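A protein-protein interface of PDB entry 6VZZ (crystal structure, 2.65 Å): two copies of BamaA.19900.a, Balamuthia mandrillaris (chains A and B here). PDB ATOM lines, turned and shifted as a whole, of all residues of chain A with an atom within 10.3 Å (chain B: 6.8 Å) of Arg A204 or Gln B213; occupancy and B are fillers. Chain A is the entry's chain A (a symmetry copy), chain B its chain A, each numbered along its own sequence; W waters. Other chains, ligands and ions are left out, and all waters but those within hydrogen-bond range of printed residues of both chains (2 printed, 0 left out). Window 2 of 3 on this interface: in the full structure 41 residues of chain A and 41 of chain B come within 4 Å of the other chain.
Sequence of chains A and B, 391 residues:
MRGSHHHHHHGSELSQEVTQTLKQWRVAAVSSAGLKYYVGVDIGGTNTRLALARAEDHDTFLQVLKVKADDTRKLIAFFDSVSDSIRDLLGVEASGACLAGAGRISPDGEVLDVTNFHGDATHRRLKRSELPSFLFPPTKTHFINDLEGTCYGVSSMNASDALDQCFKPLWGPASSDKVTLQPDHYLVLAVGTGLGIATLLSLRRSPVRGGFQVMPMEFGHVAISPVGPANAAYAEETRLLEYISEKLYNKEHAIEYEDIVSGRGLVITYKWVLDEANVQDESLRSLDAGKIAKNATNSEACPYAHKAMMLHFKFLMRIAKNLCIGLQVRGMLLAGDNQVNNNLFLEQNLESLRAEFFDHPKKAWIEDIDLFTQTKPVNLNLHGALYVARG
Leu A201 touches Leu B203, and with the chains exchanged Leu A203 touches Leu B201. Leu A201 touches Met B215, and with the chains exchanged Met A215 touches Leu B201. Leu A203 touches Val B214, and with the chains exchanged Val A214 touches Leu B203. Gln A213 touches its own counterpart, Gln B213.
Water W1 bridges N of Arg B204 (2.9 Å) and NE2 of Gln A213 (3.1 Å). Water W2 lies within hydrogen-bond range of the backbone NH of Arg A204 and the side-chain amide nitrogen of Gln B213.
Of the 14 printed residues of chain B, 6 touch a printed residue of chain A. Printed residues of chain B that touch a printed residue of chain A: Leu B201, Leu B203, Arg B204, Gln B213, Val B214 and Met B215. Hydrophobic or aromatic side chains of chain A that line the printed part of chain B: Leu A201, Leu A203 and Met A215. Among the printed residues, 10 pairs touch across the chains. Among the printed residues, no Asp or Glu carboxylate lies within 4 Å of a Lys or Arg side-chain nitrogen of the other chain.
The backbone NH of Leu B201 lies within hydrogen-bond range of the backbone carbonyl oxygen of Gln B213, 2.7 Å away. The backbone carbonyl oxygen (O) of Thr B199 lies within hydrogen-bond range of the backbone NH (N) of Met B215 (3.0 Å). N of Leu A201 lies within hydrogen-bond range of O of Gln A213, 2.7 Å away.
OE1 of Gln B213 sits at hydrogen-bond distance from NE2 of Gln A213, at 3.0 Å.
His A185 touches none of the printed residues of chain B. Of the printed residues of chain B, Leu A201 touches Leu B201, Leu B203 and Met B215. Of chain B, only Gln B213 comes within 4 Å of Arg A204. Printed residues of chain B within 4 Å of Gln A213: Arg B204 and Gln B213. Printed residues of chain B within 4 Å of Val A214: Leu B203 (3.7 Å). Of the printed residues of chain B, Met A215 touches Leu B201. Of the printed residues of chain A, Leu B201 touches Leu A201 (3.98 Å), Leu A203 (3.9 Å) and Met A215 (3.6 Å). The nearest residue of chain B that does not touch Arg A204 is Arg B204 (4.6 Å).
Leu B201 touches Leu A201. Leu A201 touches Leu B203 (CD1 to CD1, 3.9 Å). CE of Met B215 touches CD2 of Leu A201 (3.6 Å). Leu A203 touches Leu B201 (CD1 to CD1, 3.9 Å). CD2 of Leu A203 touches O of Val B214 (3.7 Å). Arg A204 touches Gln B213. Gln A213 touches Arg B204. CD2 of Leu B203 touches O of Val A214, at 3.7 Å. Leu B201 touches Met A215 (CD2 to CE, 3.6 Å).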
ATOM      1  N   PRO A 183     -30.671  -9.502 -40.690  1.00  0.00           N
ATOM      2  CA  PRO A 183     -30.538  -9.294 -39.228  1.00  0.00           C
ATOM      3  C   PRO A 183     -29.820 -10.454 -38.547  1.00  0.00           C
ATOM      4  O   PRO A 183     -30.381 -11.233 -37.761  1.00  0.00           O
ATOM      5  CB  PRO A 183     -31.999  -9.149 -38.775  1.00  0.00           C
ATOM      6  CG  PRO A 183     -32.826  -9.066 -40.017  1.00  0.00           C
ATOM      7  CD  PRO A 183     -32.062  -9.785 -41.073  1.00  0.00           C
ATOM      8  N   ASP A 184     -28.538 -10.585 -38.867  1.00  0.00           N
ATOM      9  CA  ASP A 184     -27.635 -11.540 -38.236  1.00  0.00           C
ATOM     10  C   ASP A 184     -26.339 -10.791 -37.956  1.00  0.00           C
ATOM     11  O   ASP A 184     -26.285  -9.566 -38.098  1.00  0.00           O
ATOM     12  CB  ASP A 184     -27.458 -12.784 -39.118  1.00  0.00           C
ATOM     13  CG  ASP A 184     -28.753 -13.572 -39.279  1.00  0.00           C
ATOM     14  OD1 ASP A 184     -29.453 -13.814 -38.264  1.00  0.00           O
ATOM     15  OD2 ASP A 184     -29.089 -13.946 -40.423  1.00  0.00           O
ATOM     16  N   HIS A 185     -25.294 -11.497 -37.519  1.00  0.00           N
ATOM     17  CA  HIS A 185     -24.028 -10.824 -37.260  1.00  0.00           C
ATOM     18  C   HIS A 185     -23.196 -10.781 -38.522  1.00  0.00           C
ATOM     19  O   HIS A 185     -23.240 -11.698 -39.344  1.00  0.00           O
ATOM     20  CB  HIS A 185     -23.219 -11.514 -36.166  1.00  0.00           C
ATOM     21  CG  HIS A 185     -24.027 -11.909 -34.978  1.00  0.00           C
ATOM     22  ND1 HIS A 185     -24.898 -11.047 -34.348  1.00  0.00           N
ATOM     23  CD2 HIS A 185     -24.095 -13.077 -34.299  1.00  0.00           C
ATOM     24  CE1 HIS A 185     -25.471 -11.666 -33.335  1.00  0.00           C
ATOM     25  NE2 HIS A 185     -25.009 -12.901 -33.289  1.00  0.00           N
ATOM     26  N   LEU A 201     -23.605  -6.592 -34.784  1.00  0.00           N
ATOM     27  CA  LEU A 201     -24.326  -7.583 -33.996  1.00  0.00           C
ATOM     28  C   LEU A 201     -25.832  -7.410 -34.145  1.00  0.00           C
ATOM     29  O   LEU A 201     -26.341  -6.284 -34.168  1.00  0.00           O
ATOM     30  CB  LEU A 201     -23.962  -7.477 -32.510  1.00  0.00           C
ATOM     31  CG  LEU A 201     -22.518  -7.736 -32.084  1.00  0.00           C
ATOM     32  CD1 LEU A 201     -22.331  -7.455 -30.609  1.00  0.00           C
ATOM     33  CD2 LEU A 201     -22.160  -9.163 -32.391  1.00  0.00           C
ATOM     34  N   SER A 202     -26.539  -8.535 -34.216  1.00  0.00           N
ATOM     35  CA  SER A 202     -27.999  -8.588 -34.136  1.00  0.00           C
ATOM     36  C   SER A 202     -28.386  -9.516 -32.988  1.00  0.00           C
ATOM     37  O   SER A 202     -28.654 -10.699 -33.209  1.00  0.00           O
ATOM     38  CB  SER A 202     -28.618  -9.074 -35.454  1.00  0.00           C
ATOM     39  OG  SER A 202     -28.817  -7.998 -36.349  1.00  0.00           O
ATOM     40  N   LEU A 203     -28.437  -8.981 -31.773  1.00  0.00           N
ATOM     41  CA  LEU A 203     -28.836  -9.756 -30.612  1.00  0.00           C
ATOM     42  C   LEU A 203     -30.283  -9.425 -30.229  1.00  0.00           C
ATOM     43  O   LEU A 203     -31.034  -8.853 -31.027  1.00  0.00           O
ATOM     44  CB  LEU A 203     -27.853  -9.483 -29.471  1.00  0.00           C
ATOM     45  CG  LEU A 203     -26.366  -9.688 -29.752  1.00  0.00           C
ATOM     46  CD1 LEU A 203     -25.537  -8.784 -28.847  1.00  0.00           C
ATOM     47  CD2 LEU A 203     -25.980 -11.144 -29.554  1.00  0.00           C
ATOM     48  N   ARG A 204     -30.661  -9.758 -28.991  1.00  0.00           N
ATOM     49  CA  ARG A 204     -32.014  -9.629 -28.417  1.00  0.00           C
ATOM     50  C   ARG A 204     -32.959 -10.697 -28.955  1.00  0.00           C
ATOM     51  O   ARG A 204     -32.920 -11.847 -28.508  1.00  0.00           O
ATOM     52  CB  ARG A 204     -32.599  -8.229 -28.648  1.00  0.00           C
ATOM     53  CG  ARG A 204     -32.084  -7.196 -27.662  1.00  0.00           C
ATOM     54  CD  ARG A 204     -32.550  -5.795 -27.998  1.00  0.00           C
ATOM     55  NE  ARG A 204     -31.828  -5.220 -29.132  1.00  0.00           N
ATOM     56  CZ  ARG A 204     -31.689  -3.910 -29.326  1.00  0.00           C
ATOM     57  NH1 ARG A 204     -32.216  -3.054 -28.456  1.00  0.00           N
ATOM     58  NH2 ARG A 204     -31.021  -3.455 -30.379  1.00  0.00           N
ATOM     59  N   GLY A 210     -34.107  -4.312 -33.069  1.00  0.00           N
ATOM     60  CA  GLY A 210     -34.308  -3.105 -33.849  1.00  0.00           C
ATOM     61  C   GLY A 210     -33.034  -2.317 -34.109  1.00  0.00           C
ATOM     62  O   GLY A 210     -32.763  -1.331 -33.415  1.00  0.00           O
ATOM     63  N   GLY A 211     -32.264  -2.749 -35.105  1.00  0.00           N
ATOM     64  CA  GLY A 211     -31.048  -2.080 -35.530  1.00  0.00           C
ATOM     65  C   GLY A 211     -29.833  -2.990 -35.436  1.00  0.00           C
ATOM     66  O   GLY A 211     -29.921  -4.165 -35.080  1.00  0.00           O
ATOM     67  N   PHE A 212     -28.678  -2.415 -35.773  1.00  0.00           N
ATOM     68  CA  PHE A 212     -27.390  -3.080 -35.621  1.00  0.00           C
ATOM     69  C   PHE A 212     -26.633  -2.473 -34.450  1.00  0.00           C
ATOM     70  O   PHE A 212     -26.491  -1.250 -34.364  1.00  0.00           O
ATOM     71  CB  PHE A 212     -26.541  -2.952 -36.887  1.00  0.00           C
ATOM     72  CG  PHE A 212     -26.739  -4.068 -37.859  1.00  0.00           C
ATOM     73  CD1 PHE A 212     -26.637  -5.385 -37.447  1.00  0.00           C
ATOM     74  CD2 PHE A 212     -27.048  -3.804 -39.188  1.00  0.00           C
ATOM     75  CE1 PHE A 212     -26.834  -6.423 -38.347  1.00  0.00           C
ATOM     76  CE2 PHE A 212     -27.244  -4.832 -40.094  1.00  0.00           C
ATOM     77  CZ  PHE A 212     -27.140  -6.144 -39.672  1.00  0.00           C
ATOM     78  N   GLN A 213     -26.137  -3.322 -33.560  1.00  0.00           N
ATOM     79  CA  GLN A 213     -25.208  -2.892 -32.528  1.00  0.00           C
ATOM     80  C   GLN A 213     -23.783  -3.140 -33.010  1.00  0.00           C
ATOM     81  O   GLN A 213     -23.506  -4.129 -33.693  1.00  0.00           O
ATOM     82  CB  GLN A 213     -25.471  -3.619 -31.205  1.00  0.00           C
ATOM     83  CG  GLN A 213     -26.792  -3.218 -30.538  1.00  0.00           C
ATOM     84  CD  GLN A 213     -27.007  -3.915 -29.205  1.00  0.00           C
ATOM     85  OE1 GLN A 213     -27.435  -5.067 -29.149  1.00  0.00           O
ATOM     86  NE2 GLN A 213     -26.689  -3.221 -28.122  1.00  0.00           N
ATOM     87  N   VAL A 214     -22.889  -2.222 -32.684  1.00  0.00           N
ATOM     88  CA  VAL A 214     -21.490  -2.314 -33.074  1.00  0.00           C
ATOM     89  C   VAL A 214     -20.693  -2.790 -31.872  1.00  0.00           C
ATOM     90  O   VAL A 214     -20.841  -2.252 -30.765  1.00  0.00           O
ATOM     91  CB  VAL A 214     -20.964  -0.963 -33.585  1.00  0.00           C
ATOM     92  CG1 VAL A 214     -19.506  -1.077 -34.017  1.00  0.00           C
ATOM     93  CG2 VAL A 214     -21.819  -0.456 -34.734  1.00  0.00           C
ATOM     94  N   MET A 215     -19.847  -3.801 -32.085  1.00  0.00           N
ATOM     95  CA  MET A 215     -18.900  -4.187 -31.064  1.00  0.00           C
ATOM     96  C   MET A 215     -17.483  -3.945 -31.559  1.00  0.00           C
ATOM     97  O   MET A 215     -17.057  -4.589 -32.530  1.00  0.00           O
ATOM     98  CB  MET A 215     -19.076  -5.643 -30.662  1.00  0.00           C
ATOM     99  CG  MET A 215     -18.263  -5.962 -29.426  1.00  0.00           C
ATOM    100  SD  MET A 215     -18.256  -7.689 -28.963  1.00  0.00           S
ATOM    101  CE  MET A 215     -17.124  -7.593 -27.555  1.00  0.00           C
ATOM    102  N   CYS B 151     -24.208 -17.712 -18.985  1.00  0.00           N
ATOM    103  CA  CYS B 151     -24.165 -16.266 -18.823  1.00  0.00           C
ATOM    104  C   CYS B 151     -25.441 -15.736 -18.176  1.00  0.00           C
ATOM    105  O   CYS B 151     -25.375 -14.886 -17.275  1.00  0.00           O
ATOM    106  CB  CYS B 151     -23.904 -15.600 -20.169  1.00  0.00           C
ATOM    107  SG  CYS B 151     -22.272 -16.034 -20.811  1.00  0.00           S
ATOM    108  N   TYR B 152     -26.610 -16.226 -18.603  1.00  0.00           N
ATOM    109  CA  TYR B 152     -27.841 -15.772 -17.962  1.00  0.00           C
ATOM    110  C   TYR B 152     -27.855 -16.152 -16.490  1.00  0.00           C
ATOM    111  O   TYR B 152     -28.315 -15.375 -15.642  1.00  0.00           O
ATOM    112  CB  TYR B 152     -29.066 -16.336 -18.681  1.00  0.00           C
ATOM    113  CG  TYR B 152     -29.336 -15.670 -20.002  1.00  0.00           C
ATOM    114  CD1 TYR B 152     -29.749 -14.339 -20.058  1.00  0.00           C
ATOM    115  CD2 TYR B 152     -29.177 -16.362 -21.194  1.00  0.00           C
ATOM    116  CE1 TYR B 152     -30.003 -13.720 -21.271  1.00  0.00           C
ATOM    117  CE2 TYR B 152     -29.414 -15.749 -22.413  1.00  0.00           C
ATOM    118  CZ  TYR B 152     -29.829 -14.432 -22.443  1.00  0.00           C
ATOM    119  OH  TYR B 152     -30.071 -13.828 -23.650  1.00  0.00           O
ATOM    120  N   SER B 155     -25.417 -13.641 -14.889  1.00  0.00           N
ATOM    121  CA  SER B 155     -26.042 -12.324 -14.831  1.00  0.00           C
ATOM    122  C   SER B 155     -27.139 -12.288 -13.779  1.00  0.00           C
ATOM    123  O   SER B 155     -27.268 -11.310 -13.032  1.00  0.00           O
ATOM    124  CB  SER B 155     -26.596 -11.950 -16.203  1.00  0.00           C
ATOM    125  OG  SER B 155     -27.306 -10.717 -16.150  1.00  0.00           O
ATOM    126  N   THR B 199     -19.820 -14.587 -24.023  1.00  0.00           N
ATOM    127  CA  THR B 199     -19.392 -13.294 -23.499  1.00  0.00           C
ATOM    128  C   THR B 199     -20.583 -12.518 -22.961  1.00  0.00           C
ATOM    129  O   THR B 199     -21.605 -12.388 -23.641  1.00  0.00           O
ATOM    130  CB  THR B 199     -18.687 -12.452 -24.571  1.00  0.00           C
ATOM    131  OG1 THR B 199     -17.574 -13.179 -25.094  1.00  0.00           O
ATOM    132  CG2 THR B 199     -18.180 -11.128 -23.981  1.00  0.00           C
ATOM    133  N   LEU B 200     -20.440 -11.995 -21.745  1.00  0.00           N
ATOM    134  CA  LEU B 200     -21.384 -11.033 -21.186  1.00  0.00           C
ATOM    135  C   LEU B 200     -21.000  -9.647 -21.686  1.00  0.00           C
ATOM    136  O   LEU B 200     -19.892  -9.179 -21.418  1.00  0.00           O
ATOM    137  CB  LEU B 200     -21.367 -11.091 -19.657  1.00  0.00           C
ATOM    138  CG  LEU B 200     -22.019 -12.307 -18.980  1.00  0.00           C
ATOM    139  CD1 LEU B 200     -21.532 -12.484 -17.553  1.00  0.00           C
ATOM    140  CD2 LEU B 200     -23.539 -12.178 -18.998  1.00  0.00           C
ATOM    141  N   LEU B 201     -21.900  -8.998 -22.416  1.00  0.00           N
ATOM    142  CA  LEU B 201     -21.614  -7.740 -23.092  1.00  0.00           C
ATOM    143  C   LEU B 201     -22.285  -6.572 -22.381  1.00  0.00           C
ATOM    144  O   LEU B 201     -23.432  -6.678 -21.932  1.00  0.00           O
ATOM    145  CB  LEU B 201     -22.094  -7.774 -24.548  1.00  0.00           C
ATOM    146  CG  LEU B 201     -21.471  -8.788 -25.506  1.00  0.00           C
ATOM    147  CD1 LEU B 201     -22.165  -8.758 -26.851  1.00  0.00           C
ATOM    148  CD2 LEU B 201     -20.009  -8.482 -25.668  1.00  0.00           C
ATOM    149  N   SER B 202     -21.574  -5.450 -22.312  1.00  0.00           N
ATOM    150  CA  SER B 202     -22.117  -4.163 -21.876  1.00  0.00           C
ATOM    151  C   SER B 202     -21.883  -3.141 -22.985  1.00  0.00           C
ATOM    152  O   SER B 202     -20.900  -2.399 -22.948  1.00  0.00           O
ATOM    153  CB  SER B 202     -21.470  -3.695 -20.565  1.00  0.00           C
ATOM    154  OG  SER B 202     -22.144  -4.233 -19.445  1.00  0.00           O
ATOM    155  N   LEU B 203     -22.792  -3.085 -23.952  1.00  0.00           N
ATOM    156  CA  LEU B 203     -22.699  -2.122 -25.035  1.00  0.00           C
ATOM    157  C   LEU B 203     -23.672  -0.963 -24.794  1.00  0.00           C
ATOM    158  O   LEU B 203     -24.163  -0.770 -23.676  1.00  0.00           O
ATOM    159  CB  LEU B 203     -22.961  -2.839 -26.361  1.00  0.00           C
ATOM    160  CG  LEU B 203     -22.116  -4.070 -26.682  1.00  0.00           C
ATOM    161  CD1 LEU B 203     -22.890  -5.007 -27.600  1.00  0.00           C
ATOM    162  CD2 LEU B 203     -20.798  -3.663 -27.318  1.00  0.00           C
ATOM    163  N   ARG B 204     -23.975  -0.211 -25.857  1.00  0.00           N
ATOM    164  CA  ARG B 204     -24.808   1.007 -25.868  1.00  0.00           C
ATOM    165  C   ARG B 204     -24.069   2.202 -25.277  1.00  0.00           C
ATOM    166  O   ARG B 204     -23.233   2.814 -25.949  1.00  0.00           O
ATOM    167  CB  ARG B 204     -26.143   0.789 -25.143  1.00  0.00           C
ATOM    168  CG  ARG B 204     -27.177   0.075 -25.995  1.00  0.00           C
ATOM    169  CD  ARG B 204     -28.430  -0.267 -25.216  1.00  0.00           C
ATOM    170  NE  ARG B 204     -28.238  -1.405 -24.317  1.00  0.00           N
ATOM    171  CZ  ARG B 204     -29.232  -2.188 -23.903  1.00  0.00           C
ATOM    172  NH1 ARG B 204     -30.474  -1.955 -24.317  1.00  0.00           N
ATOM    173  NH2 ARG B 204     -28.989  -3.205 -23.085  1.00  0.00           N
ATOM    174  N   GLY B 211     -28.382  -3.519 -18.195  1.00  0.00           N
ATOM    175  CA  GLY B 211     -28.334  -4.965 -18.096  1.00  0.00           C
ATOM    176  C   GLY B 211     -27.126  -5.548 -18.813  1.00  0.00           C
ATOM    177  O   GLY B 211     -26.286  -4.836 -19.363  1.00  0.00           O
ATOM    178  N   PHE B 212     -27.053  -6.879 -18.792  1.00  0.00           N
ATOM    179  CA  PHE B 212     -26.047  -7.627 -19.536  1.00  0.00           C
ATOM    180  C   PHE B 212     -26.691  -8.303 -20.736  1.00  0.00           C
ATOM    181  O   PHE B 212     -27.709  -8.986 -20.597  1.00  0.00           O
ATOM    182  CB  PHE B 212     -25.378  -8.689 -18.661  1.00  0.00           C
ATOM    183  CG  PHE B 212     -24.157  -8.203 -17.952  1.00  0.00           C
ATOM    184  CD1 PHE B 212     -23.143  -7.572 -18.652  1.00  0.00           C
ATOM    185  CD2 PHE B 212     -24.028  -8.357 -16.577  1.00  0.00           C
ATOM    186  CE1 PHE B 212     -22.014  -7.109 -17.992  1.00  0.00           C
ATOM    187  CE2 PHE B 212     -22.904  -7.899 -15.910  1.00  0.00           C
ATOM    188  CZ  PHE B 212     -21.897  -7.272 -16.618  1.00  0.00           C
ATOM    189  N   GLN B 213     -26.094  -8.127 -21.907  1.00  0.00           N
ATOM    190  CA  GLN B 213     -26.472  -8.897 -23.081  1.00  0.00           C
ATOM    191  C   GLN B 213     -25.542 -10.098 -23.206  1.00  0.00           C
ATOM    192  O   GLN B 213     -24.350 -10.014 -22.902  1.00  0.00           O
ATOM    193  CB  GLN B 213     -26.425  -8.037 -24.349  1.00  0.00           C
ATOM    194  CG  GLN B 213     -27.511  -6.955 -24.396  1.00  0.00           C
ATOM    195  CD  GLN B 213     -27.475  -6.148 -25.683  1.00  0.00           C
ATOM    196  OE1 GLN B 213     -26.677  -5.224 -25.834  1.00  0.00           O
ATOM    197  NE2 GLN B 213     -28.330  -6.511 -26.627  1.00  0.00           N
ATOM    198  N   VAL B 214     -26.098 -11.225 -23.619  1.00  0.00           N
ATOM    199  CA  VAL B 214     -25.344 -12.459 -23.783  1.00  0.00           C
ATOM    200  C   VAL B 214     -25.061 -12.648 -25.263  1.00  0.00           C
ATOM    201  O   VAL B 214     -25.970 -12.535 -26.098  1.00  0.00           O
ATOM    202  CB  VAL B 214     -26.112 -13.661 -23.211  1.00  0.00           C
ATOM    203  CG1 VAL B 214     -25.301 -14.944 -23.363  1.00  0.00           C
ATOM    204  CG2 VAL B 214     -26.461 -13.426 -21.751  1.00  0.00           C
ATOM    205  N   MET B 215     -23.799 -12.934 -25.594  1.00  0.00           N
ATOM    206  CA  MET B 215     -23.471 -13.334 -26.944  1.00  0.00           C
ATOM    207  C   MET B 215     -22.957 -14.765 -26.946  1.00  0.00           C
ATOM    208  O   MET B 215     -21.899 -15.035 -26.357  1.00  0.00           O
ATOM    209  CB  MET B 215     -22.442 -12.403 -27.565  1.00  0.00           C
ATOM    210  CG  MET B 215     -22.298 -12.673 -29.047  1.00  0.00           C
ATOM    211  SD  MET B 215     -20.989 -11.757 -29.849  1.00  0.00           S
ATOM    212  CE  MET B 215     -21.139 -12.458 -31.511  1.00  0.00           C
HETATM  213  O   HOH W   1     -24.900  -0.715 -28.589  1.00  0.00           O
HETATM  214  O   HOH W   2     -29.612  -9.330 -26.291  1.00  0.00           O
